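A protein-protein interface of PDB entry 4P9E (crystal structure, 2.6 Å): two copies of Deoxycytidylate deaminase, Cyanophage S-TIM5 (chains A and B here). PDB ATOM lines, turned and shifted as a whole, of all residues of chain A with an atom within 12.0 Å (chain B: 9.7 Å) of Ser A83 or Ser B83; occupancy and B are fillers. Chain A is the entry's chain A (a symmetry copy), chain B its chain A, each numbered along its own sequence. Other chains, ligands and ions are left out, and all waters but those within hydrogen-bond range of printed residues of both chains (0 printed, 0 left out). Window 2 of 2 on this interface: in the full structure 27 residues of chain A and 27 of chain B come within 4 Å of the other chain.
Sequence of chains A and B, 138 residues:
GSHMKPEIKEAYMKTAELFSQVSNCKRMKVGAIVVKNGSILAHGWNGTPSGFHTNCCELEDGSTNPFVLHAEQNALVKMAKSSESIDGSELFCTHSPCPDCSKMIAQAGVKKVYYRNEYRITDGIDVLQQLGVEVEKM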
ATOM      1  N   VAL A  34     -15.991  11.825  -7.512  1.00  0.00           N
ATOM      2  CA  VAL A  34     -15.998  11.730  -6.054  1.00  0.00           C
ATOM      3  C   VAL A  34     -16.172  13.107  -5.414  1.00  0.00           C
ATOM      4  O   VAL A  34     -15.489  14.066  -5.766  1.00  0.00           O
ATOM      5  CB  VAL A  34     -14.758  10.982  -5.494  1.00  0.00           C
ATOM      6  CG1 VAL A  34     -14.721  11.068  -3.974  1.00  0.00           C
ATOM      7  CG2 VAL A  34     -14.801   9.516  -5.915  1.00  0.00           C
ATOM      8  N   LYS A  36     -16.628  15.194  -1.621  1.00  0.00           N
ATOM      9  CA  LYS A  36     -16.556  15.164  -0.168  1.00  0.00           C
ATOM     10  C   LYS A  36     -16.373  16.578   0.357  1.00  0.00           C
ATOM     11  O   LYS A  36     -15.610  17.372  -0.208  1.00  0.00           O
ATOM     12  CB  LYS A  36     -15.407  14.266   0.265  1.00  0.00           C
ATOM     13  CG  LYS A  36     -15.300  14.025   1.735  1.00  0.00           C
ATOM     14  CD  LYS A  36     -14.192  13.041   1.983  1.00  0.00           C
ATOM     15  CE  LYS A  36     -13.854  12.913   3.451  1.00  0.00           C
ATOM     16  NZ  LYS A  36     -12.554  12.190   3.649  1.00  0.00           N
ATOM     17  N   ASN A  37     -17.094  16.894   1.431  1.00  0.00           N
ATOM     18  CA  ASN A  37     -17.022  18.213   2.063  1.00  0.00           C
ATOM     19  C   ASN A  37     -17.133  19.388   1.093  1.00  0.00           C
ATOM     20  O   ASN A  37     -16.405  20.367   1.212  1.00  0.00           O
ATOM     21  CB  ASN A  37     -15.728  18.351   2.856  1.00  0.00           C
ATOM     22  CG  ASN A  37     -15.515  17.208   3.830  1.00  0.00           C
ATOM     23  OD1 ASN A  37     -16.473  16.584   4.296  1.00  0.00           O
ATOM     24  ND2 ASN A  37     -14.255  16.918   4.135  1.00  0.00           N
ATOM     25  N   SER A  39     -16.435  19.426  -2.109  1.00  0.00           N
ATOM     26  CA  SER A  39     -15.375  19.494  -3.079  1.00  0.00           C
ATOM     27  C   SER A  39     -15.238  18.211  -3.909  1.00  0.00           C
ATOM     28  O   SER A  39     -15.259  17.102  -3.367  1.00  0.00           O
ATOM     29  CB  SER A  39     -14.073  19.804  -2.358  1.00  0.00           C
ATOM     30  OG  SER A  39     -12.996  19.834  -3.272  1.00  0.00           O
ATOM     31  N   ILE A  40     -15.100  18.371  -5.223  1.00  0.00           N
ATOM     32  CA  ILE A  40     -14.718  17.256  -6.086  1.00  0.00           C
ATOM     33  C   ILE A  40     -13.294  16.834  -5.750  1.00  0.00           C
ATOM     34  O   ILE A  40     -12.421  17.677  -5.607  1.00  0.00           O
ATOM     35  CB  ILE A  40     -14.755  17.647  -7.578  1.00  0.00           C
ATOM     36  CG1 ILE A  40     -16.126  18.179  -7.957  1.00  0.00           C
ATOM     37  CG2 ILE A  40     -14.391  16.462  -8.463  1.00  0.00           C
ATOM     38  CD1 ILE A  40     -16.181  18.666  -9.374  1.00  0.00           C
ATOM     39  N   LEU A  41     -13.056  15.538  -5.620  1.00  0.00           N
ATOM     40  CA  LEU A  41     -11.726  15.063  -5.288  1.00  0.00           C
ATOM     41  C   LEU A  41     -11.135  14.187  -6.372  1.00  0.00           C
ATOM     42  O   LEU A  41      -9.932  14.030  -6.447  1.00  0.00           O
ATOM     43  CB  LEU A  41     -11.745  14.294  -3.975  1.00  0.00           C
ATOM     44  CG  LEU A  41     -12.303  15.049  -2.782  1.00  0.00           C
ATOM     45  CD1 LEU A  41     -12.296  14.106  -1.609  1.00  0.00           C
ATOM     46  CD2 LEU A  41     -11.534  16.346  -2.498  1.00  0.00           C
ATOM     47  N   ALA A  42     -11.979  13.611  -7.208  1.00  0.00           N
ATOM     48  CA  ALA A  42     -11.521  12.688  -8.239  1.00  0.00           C
ATOM     49  C   ALA A  42     -12.577  12.557  -9.316  1.00  0.00           C
ATOM     50  O   ALA A  42     -13.772  12.735  -9.064  1.00  0.00           O
ATOM     51  CB  ALA A  42     -11.215  11.306  -7.643  1.00  0.00           C
ATOM     52  N   ALA A  75     -11.660   6.481 -10.678  1.00  0.00           N
ATOM     53  CA  ALA A  75     -11.818   7.411  -9.579  1.00  0.00           C
ATOM     54  C   ALA A  75     -11.142   6.880  -8.304  1.00  0.00           C
ATOM     55  O   ALA A  75     -10.334   7.570  -7.677  1.00  0.00           O
ATOM     56  CB  ALA A  75     -13.305   7.702  -9.339  1.00  0.00           C
ATOM     57  N   LEU A  76     -11.475   5.646  -7.943  1.00  0.00           N
ATOM     58  CA  LEU A  76     -10.860   4.958  -6.821  1.00  0.00           C
ATOM     59  C   LEU A  76      -9.332   4.932  -6.865  1.00  0.00           C
ATOM     60  O   LEU A  76      -8.667   5.204  -5.871  1.00  0.00           O
ATOM     61  CB  LEU A  76     -11.377   3.527  -6.775  1.00  0.00           C
ATOM     62  CG  LEU A  76     -10.866   2.692  -5.597  1.00  0.00           C
ATOM     63  CD1 LEU A  76     -11.292   3.303  -4.280  1.00  0.00           C
ATOM     64  CD2 LEU A  76     -11.383   1.287  -5.716  1.00  0.00           C
ATOM     65  N   VAL A  77      -8.766   4.577  -8.010  1.00  0.00           N
ATOM     66  CA  VAL A  77      -7.313   4.584  -8.136  1.00  0.00           C
ATOM     67  C   VAL A  77      -6.736   5.997  -7.958  1.00  0.00           C
ATOM     68  O   VAL A  77      -5.698   6.174  -7.329  1.00  0.00           O
ATOM     69  CB  VAL A  77      -6.841   3.901  -9.455  1.00  0.00           C
ATOM     70  CG1 VAL A  77      -5.473   4.404  -9.891  1.00  0.00           C
ATOM     71  CG2 VAL A  77      -6.837   2.382  -9.289  1.00  0.00           C
ATOM     72  N   LYS A  78      -7.421   7.002  -8.482  1.00  0.00           N
ATOM     73  CA  LYS A  78      -6.991   8.380  -8.246  1.00  0.00           C
ATOM     74  C   LYS A  78      -7.025   8.753  -6.771  1.00  0.00           C
ATOM     75  O   LYS A  78      -6.138   9.467  -6.302  1.00  0.00           O
ATOM     76  CB  LYS A  78      -7.804   9.376  -9.075  1.00  0.00           C
ATOM     77  CG  LYS A  78      -7.361   9.440 -10.501  1.00  0.00           C
ATOM     78  CD  LYS A  78      -8.283  10.262 -11.357  1.00  0.00           C
ATOM     79  CE  LYS A  78      -7.929  10.090 -12.832  1.00  0.00           C
ATOM     80  NZ  LYS A  78      -8.830  10.862 -13.717  1.00  0.00           N
ATOM     81  N   MET A  79      -8.035   8.275  -6.048  1.00  0.00           N
ATOM     82  CA  MET A  79      -8.121   8.485  -4.608  1.00  0.00           C
ATOM     83  C   MET A  79      -6.979   7.827  -3.875  1.00  0.00           C
ATOM     84  O   MET A  79      -6.492   8.371  -2.915  1.00  0.00           O
ATOM     85  CB  MET A  79      -9.446   7.988  -4.026  1.00  0.00           C
ATOM     86  CG  MET A  79     -10.631   8.837  -4.404  1.00  0.00           C
ATOM     87  SD  MET A  79     -10.338  10.594  -4.156  1.00  0.00           S
ATOM     88  CE  MET A  79     -10.447  10.768  -2.382  1.00  0.00           C
ATOM     89  N   ALA A  80      -6.562   6.653  -4.324  1.00  0.00           N
ATOM     90  CA  ALA A  80      -5.398   5.991  -3.751  1.00  0.00           C
ATOM     91  C   ALA A  80      -4.091   6.770  -3.952  1.00  0.00           C
ATOM     92  O   ALA A  80      -3.186   6.658  -3.145  1.00  0.00           O
ATOM     93  CB  ALA A  80      -5.278   4.598  -4.289  1.00  0.00           C
ATOM     94  N   LYS A  81      -3.992   7.564  -5.011  1.00  0.00           N
ATOM     95  CA  LYS A  81      -2.809   8.408  -5.232  1.00  0.00           C
ATOM     96  C   LYS A  81      -2.986   9.821  -4.690  1.00  0.00           C
ATOM     97  O   LYS A  81      -2.079  10.646  -4.782  1.00  0.00           O
ATOM     98  CB  LYS A  81      -2.448   8.493  -6.714  1.00  0.00           C
ATOM     99  CG  LYS A  81      -2.266   7.160  -7.373  1.00  0.00           C
ATOM    100  CD  LYS A  81      -1.857   7.311  -8.824  1.00  0.00           C
ATOM    101  CE  LYS A  81      -2.951   7.949  -9.638  1.00  0.00           C
ATOM    102  NZ  LYS A  81      -2.763   7.741 -11.123  1.00  0.00           N
ATOM    103  N   SER A  82      -4.168  10.099  -4.152  1.00  0.00           N
ATOM    104  CA  SER A  82      -4.478  11.384  -3.544  1.00  0.00           C
ATOM    105  C   SER A  82      -3.981  11.369  -2.099  1.00  0.00           C
ATOM    106  O   SER A  82      -3.609  10.336  -1.589  1.00  0.00           O
ATOM    107  CB  SER A  82      -5.998  11.597  -3.592  1.00  0.00           C
ATOM    108  OG  SER A  82      -6.413  12.749  -2.882  1.00  0.00           O
ATOM    109  N   SER A  83      -3.980  12.514  -1.438  1.00  0.00           N
ATOM    110  CA  SER A  83      -3.653  12.561  -0.024  1.00  0.00           C
ATOM    111  C   SER A  83      -4.929  12.608   0.802  1.00  0.00           C
ATOM    112  O   SER A  83      -4.897  12.625   2.031  1.00  0.00           O
ATOM    113  CB  SER A  83      -2.831  13.808   0.269  1.00  0.00           C
ATOM    114  OG  SER A  83      -2.140  14.218  -0.895  1.00  0.00           O
ATOM    115  N   GLU A  84      -6.050  12.629   0.106  1.00  0.00           N
ATOM    116  CA  GLU A  84      -7.334  12.870   0.721  1.00  0.00           C
ATOM    117  C   GLU A  84      -8.087  11.550   0.776  1.00  0.00           C
ATOM    118  O   GLU A  84      -8.114  10.806  -0.195  1.00  0.00           O
ATOM    119  CB  GLU A  84      -8.068  13.924  -0.119  1.00  0.00           C
ATOM    120  CG  GLU A  84      -9.381  14.397   0.421  1.00  0.00           C
ATOM    121  CD  GLU A  84      -9.241  15.153   1.722  1.00  0.00           C
ATOM    122  OE1 GLU A  84      -8.671  16.270   1.698  1.00  0.00           O
ATOM    123  OE2 GLU A  84      -9.707  14.630   2.761  1.00  0.00           O
ATOM    124  N   SER A  85      -8.679  11.243   1.917  1.00  0.00           N
ATOM    125  CA  SER A  85      -9.360   9.962   2.091  1.00  0.00           C
ATOM    126  C   SER A  85     -10.664   9.855   1.295  1.00  0.00           C
ATOM    127  O   SER A  85     -11.367  10.843   1.101  1.00  0.00           O
ATOM    128  CB  SER A  85      -9.641   9.694   3.564  1.00  0.00           C
ATOM    129  OG  SER A  85     -10.373   8.498   3.710  1.00  0.00           O
ATOM    130  N   ILE A  86     -10.984   8.646   0.845  1.00  0.00           N
ATOM    131  CA  ILE A  86     -12.219   8.418   0.113  1.00  0.00           C
ATOM    132  C   ILE A  86     -13.380   8.154   1.087  1.00  0.00           C
ATOM    133  O   ILE A  86     -14.553   8.262   0.726  1.00  0.00           O
ATOM    134  CB  ILE A  86     -12.064   7.268  -0.912  1.00  0.00           C
ATOM    135  CG1 ILE A  86     -13.202   7.308  -1.935  1.00  0.00           C
ATOM    136  CG2 ILE A  86     -11.983   5.922  -0.227  1.00  0.00           C
ATOM    137  CD1 ILE A  86     -13.145   6.219  -2.955  1.00  0.00           C
ATOM    138  N   ASP A  87     -13.028   7.829   2.328  1.00  0.00           N
ATOM    139  CA  ASP A  87     -13.997   7.527   3.370  1.00  0.00           C
ATOM    140  C   ASP A  87     -14.917   8.716   3.651  1.00  0.00           C
ATOM    141  O   ASP A  87     -14.442   9.825   3.875  1.00  0.00           O
ATOM    142  CB  ASP A  87     -13.249   7.159   4.646  1.00  0.00           C
ATOM    143  CG  ASP A  87     -14.072   6.294   5.593  1.00  0.00           C
ATOM    144  OD1 ASP A  87     -15.215   5.931   5.250  1.00  0.00           O
ATOM    145  OD2 ASP A  87     -13.563   5.963   6.685  1.00  0.00           O
ATOM    146  N   SER A  89     -16.968  10.078   1.553  1.00  0.00           N
ATOM    147  CA  SER A  89     -17.294  10.793   0.334  1.00  0.00           C
ATOM    148  C   SER A  89     -18.546  10.224  -0.312  1.00  0.00           C
ATOM    149  O   SER A  89     -19.107   9.227   0.155  1.00  0.00           O
ATOM    150  CB  SER A  89     -16.149  10.679  -0.660  1.00  0.00           C
ATOM    151  OG  SER A  89     -16.064   9.353  -1.145  1.00  0.00           O
ATOM    152  N   ALA A 108     -14.583   0.993   0.691  1.00  0.00           N
ATOM    153  CA  ALA A 108     -13.882   2.275   0.690  1.00  0.00           C
ATOM    154  C   ALA A 108     -14.501   3.295   1.639  1.00  0.00           C
ATOM    155  O   ALA A 108     -13.940   4.360   1.872  1.00  0.00           O
ATOM    156  CB  ALA A 108     -13.823   2.835  -0.720  1.00  0.00           C
ATOM    157  N   LYS B  36       6.491   1.522   0.737  1.00  0.00           N
ATOM    158  CA  LYS B  36       7.024   2.715   0.097  1.00  0.00           C
ATOM    159  C   LYS B  36       7.950   3.435   1.063  1.00  0.00           C
ATOM    160  O   LYS B  36       7.658   3.546   2.261  1.00  0.00           O
ATOM    161  CB  LYS B  36       5.877   3.617  -0.334  1.00  0.00           C
ATOM    162  CG  LYS B  36       6.268   4.816  -1.134  1.00  0.00           C
ATOM    163  CD  LYS B  36       5.021   5.533  -1.568  1.00  0.00           C
ATOM    164  CE  LYS B  36       5.318   6.882  -2.183  1.00  0.00           C
ATOM    165  NZ  LYS B  36       4.072   7.709  -2.307  1.00  0.00           N
ATOM    166  N   LEU B  41       2.568   0.502   4.262  1.00  0.00           N
ATOM    167  CA  LEU B  41       1.503   1.487   4.287  1.00  0.00           C
ATOM    168  C   LEU B  41       0.127   0.855   4.317  1.00  0.00           C
ATOM    169  O   LEU B  41      -0.830   1.485   4.722  1.00  0.00           O
ATOM    170  CB  LEU B  41       1.605   2.415   3.085  1.00  0.00           C
ATOM    171  CG  LEU B  41       2.930   3.136   2.925  1.00  0.00           C
ATOM    172  CD1 LEU B  41       2.853   3.943   1.658  1.00  0.00           C
ATOM    173  CD2 LEU B  41       3.282   3.995   4.148  1.00  0.00           C
ATOM    174  N   ALA B  42       0.026  -0.387   3.881  1.00  0.00           N
ATOM    175  CA  ALA B  42      -1.263  -1.062   3.795  1.00  0.00           C
ATOM    176  C   ALA B  42      -1.054  -2.561   3.733  1.00  0.00           C
ATOM    177  O   ALA B  42      -0.018  -3.042   3.267  1.00  0.00           O
ATOM    178  CB  ALA B  42      -2.046  -0.596   2.558  1.00  0.00           C
ATOM    179  N   VAL B  77      -7.872  -0.360  -1.616  1.00  0.00           N
ATOM    180  CA  VAL B  77      -8.925   0.400  -0.953  1.00  0.00           C
ATOM    181  C   VAL B  77      -8.416   1.075   0.330  1.00  0.00           C
ATOM    182  O   VAL B  77      -8.770   2.213   0.620  1.00  0.00           O
ATOM    183  CB  VAL B  77     -10.201  -0.464  -0.716  1.00  0.00           C
ATOM    184  CG1 VAL B  77     -11.031   0.067   0.443  1.00  0.00           C
ATOM    185  CG2 VAL B  77     -11.033  -0.536  -1.995  1.00  0.00           C
ATOM    186  N   LYS B  78      -7.563   0.392   1.079  1.00  0.00           N
ATOM    187  CA  LYS B  78      -6.950   1.021   2.246  1.00  0.00           C
ATOM    188  C   LYS B  78      -6.096   2.225   1.874  1.00  0.00           C
ATOM    189  O   LYS B  78      -6.095   3.220   2.600  1.00  0.00           O
ATOM    190  CB  LYS B  78      -6.141   0.017   3.070  1.00  0.00           C
ATOM    191  CG  LYS B  78      -7.000  -0.845   3.937  1.00  0.00           C
ATOM    192  CD  LYS B  78      -6.228  -1.958   4.590  1.00  0.00           C
ATOM    193  CE  LYS B  78      -7.185  -2.945   5.254  1.00  0.00           C
ATOM    194  NZ  LYS B  78      -6.471  -4.075   5.889  1.00  0.00           N
ATOM    195  N   MET B  79      -5.381   2.137   0.755  1.00  0.00           N
ATOM    196  CA  MET B  79      -4.601   3.260   0.247  1.00  0.00           C
ATOM    197  C   MET B  79      -5.478   4.427  -0.130  1.00  0.00           C
ATOM    198  O   MET B  79      -5.098   5.552   0.077  1.00  0.00           O
ATOM    199  CB  MET B  79      -3.737   2.872  -0.955  1.00  0.00           C
ATOM    200  CG  MET B  79      -2.571   1.986  -0.602  1.00  0.00           C
ATOM    201  SD  MET B  79      -1.632   2.597   0.806  1.00  0.00           S
ATOM    202  CE  MET B  79      -0.720   3.966   0.112  1.00  0.00           C
ATOM    203  N   ALA B  80      -6.646   4.157  -0.691  1.00  0.00           N
ATOM    204  CA  ALA B  80      -7.608   5.209  -0.991  1.00  0.00           C
ATOM    205  C   ALA B  80      -8.135   5.929   0.258  1.00  0.00           C
ATOM    206  O   ALA B  80      -8.494   7.091   0.185  1.00  0.00           O
ATOM    207  CB  ALA B  80      -8.736   4.663  -1.809  1.00  0.00           C
ATOM    208  N   LYS B  81      -8.172   5.254   1.401  1.00  0.00           N
ATOM    209  CA  LYS B  81      -8.584   5.893   2.659  1.00  0.00           C
ATOM    210  C   LYS B  81      -7.402   6.413   3.467  1.00  0.00           C
ATOM    211  O   LYS B  81      -7.581   6.987   4.539  1.00  0.00           O
ATOM    212  CB  LYS B  81      -9.396   4.940   3.533  1.00  0.00           C
ATOM    213  CG  LYS B  81     -10.583   4.341   2.841  1.00  0.00           C
ATOM    214  CD  LYS B  81     -11.376   3.450   3.775  1.00  0.00           C
ATOM    215  CE  LYS B  81     -10.578   2.244   4.191  1.00  0.00           C
ATOM    216  NZ  LYS B  81     -11.445   1.147   4.764  1.00  0.00           N
ATOM    217  N   SER B  82      -6.197   6.179   2.961  1.00  0.00           N
ATOM    218  CA  SER B  82      -4.971   6.655   3.585  1.00  0.00           C
ATOM    219  C   SER B  82      -4.727   8.095   3.136  1.00  0.00           C
ATOM    220  O   SER B  82      -5.384   8.579   2.242  1.00  0.00           O
ATOM    221  CB  SER B  82      -3.812   5.748   3.148  1.00  0.00           C
ATOM    222  OG  SER B  82      -2.551   6.224   3.576  1.00  0.00           O
ATOM    223  N   SER B  83      -3.777   8.778   3.755  1.00  0.00           N
ATOM    224  CA  SER B  83      -3.391  10.102   3.298  1.00  0.00           C
ATOM    225  C   SER B  83      -2.139  10.010   2.441  1.00  0.00           C
ATOM    226  O   SER B  83      -1.642  11.009   1.923  1.00  0.00           O
ATOM    227  CB  SER B  83      -3.103  10.991   4.499  1.00  0.00           C
ATOM    228  OG  SER B  83      -3.820  10.530   5.628  1.00  0.00           O
ATOM    229  N   GLU B  84      -1.637   8.797   2.303  1.00  0.00           N
ATOM    230  CA  GLU B  84      -0.351   8.561   1.691  1.00  0.00           C
ATOM    231  C   GLU B  84      -0.588   7.978   0.306  1.00  0.00           C
ATOM    232  O   GLU B  84      -1.409   7.089   0.135  1.00  0.00           O
ATOM    233  CB  GLU B  84       0.433   7.603   2.599  1.00  0.00           C
ATOM    234  CG  GLU B  84       1.845   7.320   2.192  1.00  0.00           C
ATOM    235  CD  GLU B  84       2.732   8.540   2.273  1.00  0.00           C
ATOM    236  OE1 GLU B  84       2.988   9.012   3.407  1.00  0.00           O
ATOM    237  OE2 GLU B  84       3.176   9.021   1.203  1.00  0.00           O
ATOM    238  N   SER B  85       0.113   8.493  -0.689  1.00  0.00           N
ATOM    239  CA  SER B  85      -0.101   8.054  -2.066  1.00  0.00           C
ATOM    240  C   SER B  85       0.410   6.636  -2.337  1.00  0.00           C
ATOM    241  O   SER B  85       1.401   6.201  -1.756  1.00  0.00           O
ATOM    242  CB  SER B  85       0.544   9.022  -3.050  1.00  0.00           C
ATOM    243  OG  SER B  85       0.405   8.541  -4.368  1.00  0.00           O
ATOM    244  N   ILE B  86      -0.269   5.923  -3.230  1.00  0.00           N
ATOM    245  CA  ILE B  86       0.148   4.580  -3.597  1.00  0.00           C
ATOM    246  C   ILE B  86       1.199   4.632  -4.720  1.00  0.00           C
ATOM    247  O   ILE B  86       1.927   3.667  -4.958  1.00  0.00           O
ATOM    248  CB  ILE B  86      -1.062   3.700  -3.992  1.00  0.00           C
ATOM    249  CG1 ILE B  86      -0.673   2.220  -3.977  1.00  0.00           C
ATOM    250  CG2 ILE B  86      -1.631   4.109  -5.333  1.00  0.00           C
ATOM    251  CD1 ILE B  86      -1.778   1.294  -4.366  1.00  0.00           C
ATOM    252  N   ASP B  87       1.277   5.782  -5.384  1.00  0.00           N
ATOM    253  CA  ASP B  87       2.200   5.997  -6.488  1.00  0.00           C
ATOM    254  C   ASP B  87       3.656   5.840  -6.047  1.00  0.00           C
ATOM    255  O   ASP B  87       4.076   6.450  -5.068  1.00  0.00           O
ATOM    256  CB  ASP B  87       1.992   7.403  -7.037  1.00  0.00           C
ATOM    257  CG  ASP B  87       2.442   7.552  -8.485  1.00  0.00           C
ATOM    258  OD1 ASP B  87       2.877   6.553  -9.094  1.00  0.00           O
ATOM    259  OD2 ASP B  87       2.346   8.674  -9.022  1.00  0.00           O
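O of Ala B80 is in hydrogen-bond range of N of Ile A86. The backbone carbonyl oxygen (O) of Lys B81 is in hydrogen-bond range of the side-chain hydroxyl (OG) of Ser A85, 3.3 Å away. The backbone carbonyl oxygen (O) of Lys A81 lies within hydrogen-bond range of the side-chain hydroxyl (OG) of Ser B85 (3.3 Å). O of Ala A80 is in hydrogen-bond range of N of Ile B86, 3.0 Å away.
The side-chain carboxylate (OE2) of Glu B84 is in salt-bridge range of the side-chain amino group (NZ) of Lys B36, at 3.9 Å. The side-chain hydroxyl of Ser B85 lies within hydrogen-bond range of the backbone NH of Asp B87, 3.1 Å away. OE2 of Glu A84 lies within salt-bridge range of NZ of Lys A36, 3.9 Å away. NZ of Lys A36 is in hydrogen-bond range of O of Ser A85 (3.1 Å). OG of Ser A82 lies within hydrogen-bond range of N of Glu A84, at 3.0 Å. The side-chain hydroxyl (OG) of Ser A85 lies within hydrogen-bond range of the backbone NH (N) of Asp A87 (3.1 Å).
Among the printed residues, merely in contact across the chains: Leu A76 with Ala B80 (3.8 Å), Met A79 with Ala B80 (3.9 Å), Ala A80 with Met B79 (3.9 Å), Ala A80 with Ala B80 (3.6 Å), Ala A80 with Glu B84 (3.8 Å), Ala A80 with Ser B85 (3.6 Å), Lys A81 with Ile B86 (3.7 Å), Ser A83 with Ser B83 (3.2 Å), Glu A84 with Ala B80 (3.8 Å), Ser A85 with Ala B80 (3.6 Å), Ile A86 with Lys B81 (3.7 Å), Ala A108 with Val B77 (3.6 Å) and Ala A108 with Lys B81 (3.3 Å).
Ser A83 touches just one residue of chain B: Ser B83 (3.2 Å). Glu A84 touches just one residue of chain B: Ala B80 (3.8 Å). No residue of chain A comes within 4 Å of Ser B82. Of chain A, only Ala A80 (3.6 Å) and Lys A81 (3.3 Å) come within 4 Å of Ser B85. Printed residues of chain B within 4 Å of Ser A85: Ala B80 and Lys B81. Of the printed residues of chain B, Ala A108 touches Val B77 (3.6 Å) and Lys B81 (3.3 Å). Lys B78 touches none of the printed residues of chain A.
Of the 22 printed residues of chain A, 9 touch a printed residue of chain B. Hydrophobic or aromatic side chains of chain A that line the printed part of chain B: Leu A76, Ala A80 and Ile A86. Along chain A the printed residues that touch a printed residue of chain B span positions 76 to 108. Printed residues of chain B that touch a printed residue of chain A: Val B77, Met B79, Ala B80, Lys B81, Ser B83, Glu B84, Ser B85 and Ile B86. Hydrophobic or aromatic side chains of chain B that line the printed part of chain A: Val B77, Ala B80 and Ile B86. Among the printed residues, no Asp or Glu carboxylate lies within 4 Å of a Lys or Arg side-chain nitrogen of the other chain.
Ala A80 touches its own counterpart, Ala B80. Ala A80 touches Glu B84, and with the chains exchanged Glu A84 touches Ala B80. Lys A81 touches Ile B86, and with the chains exchanged Ile A86 touches Lys B81. Ser B83 touches its own counterpart, Ser A83.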
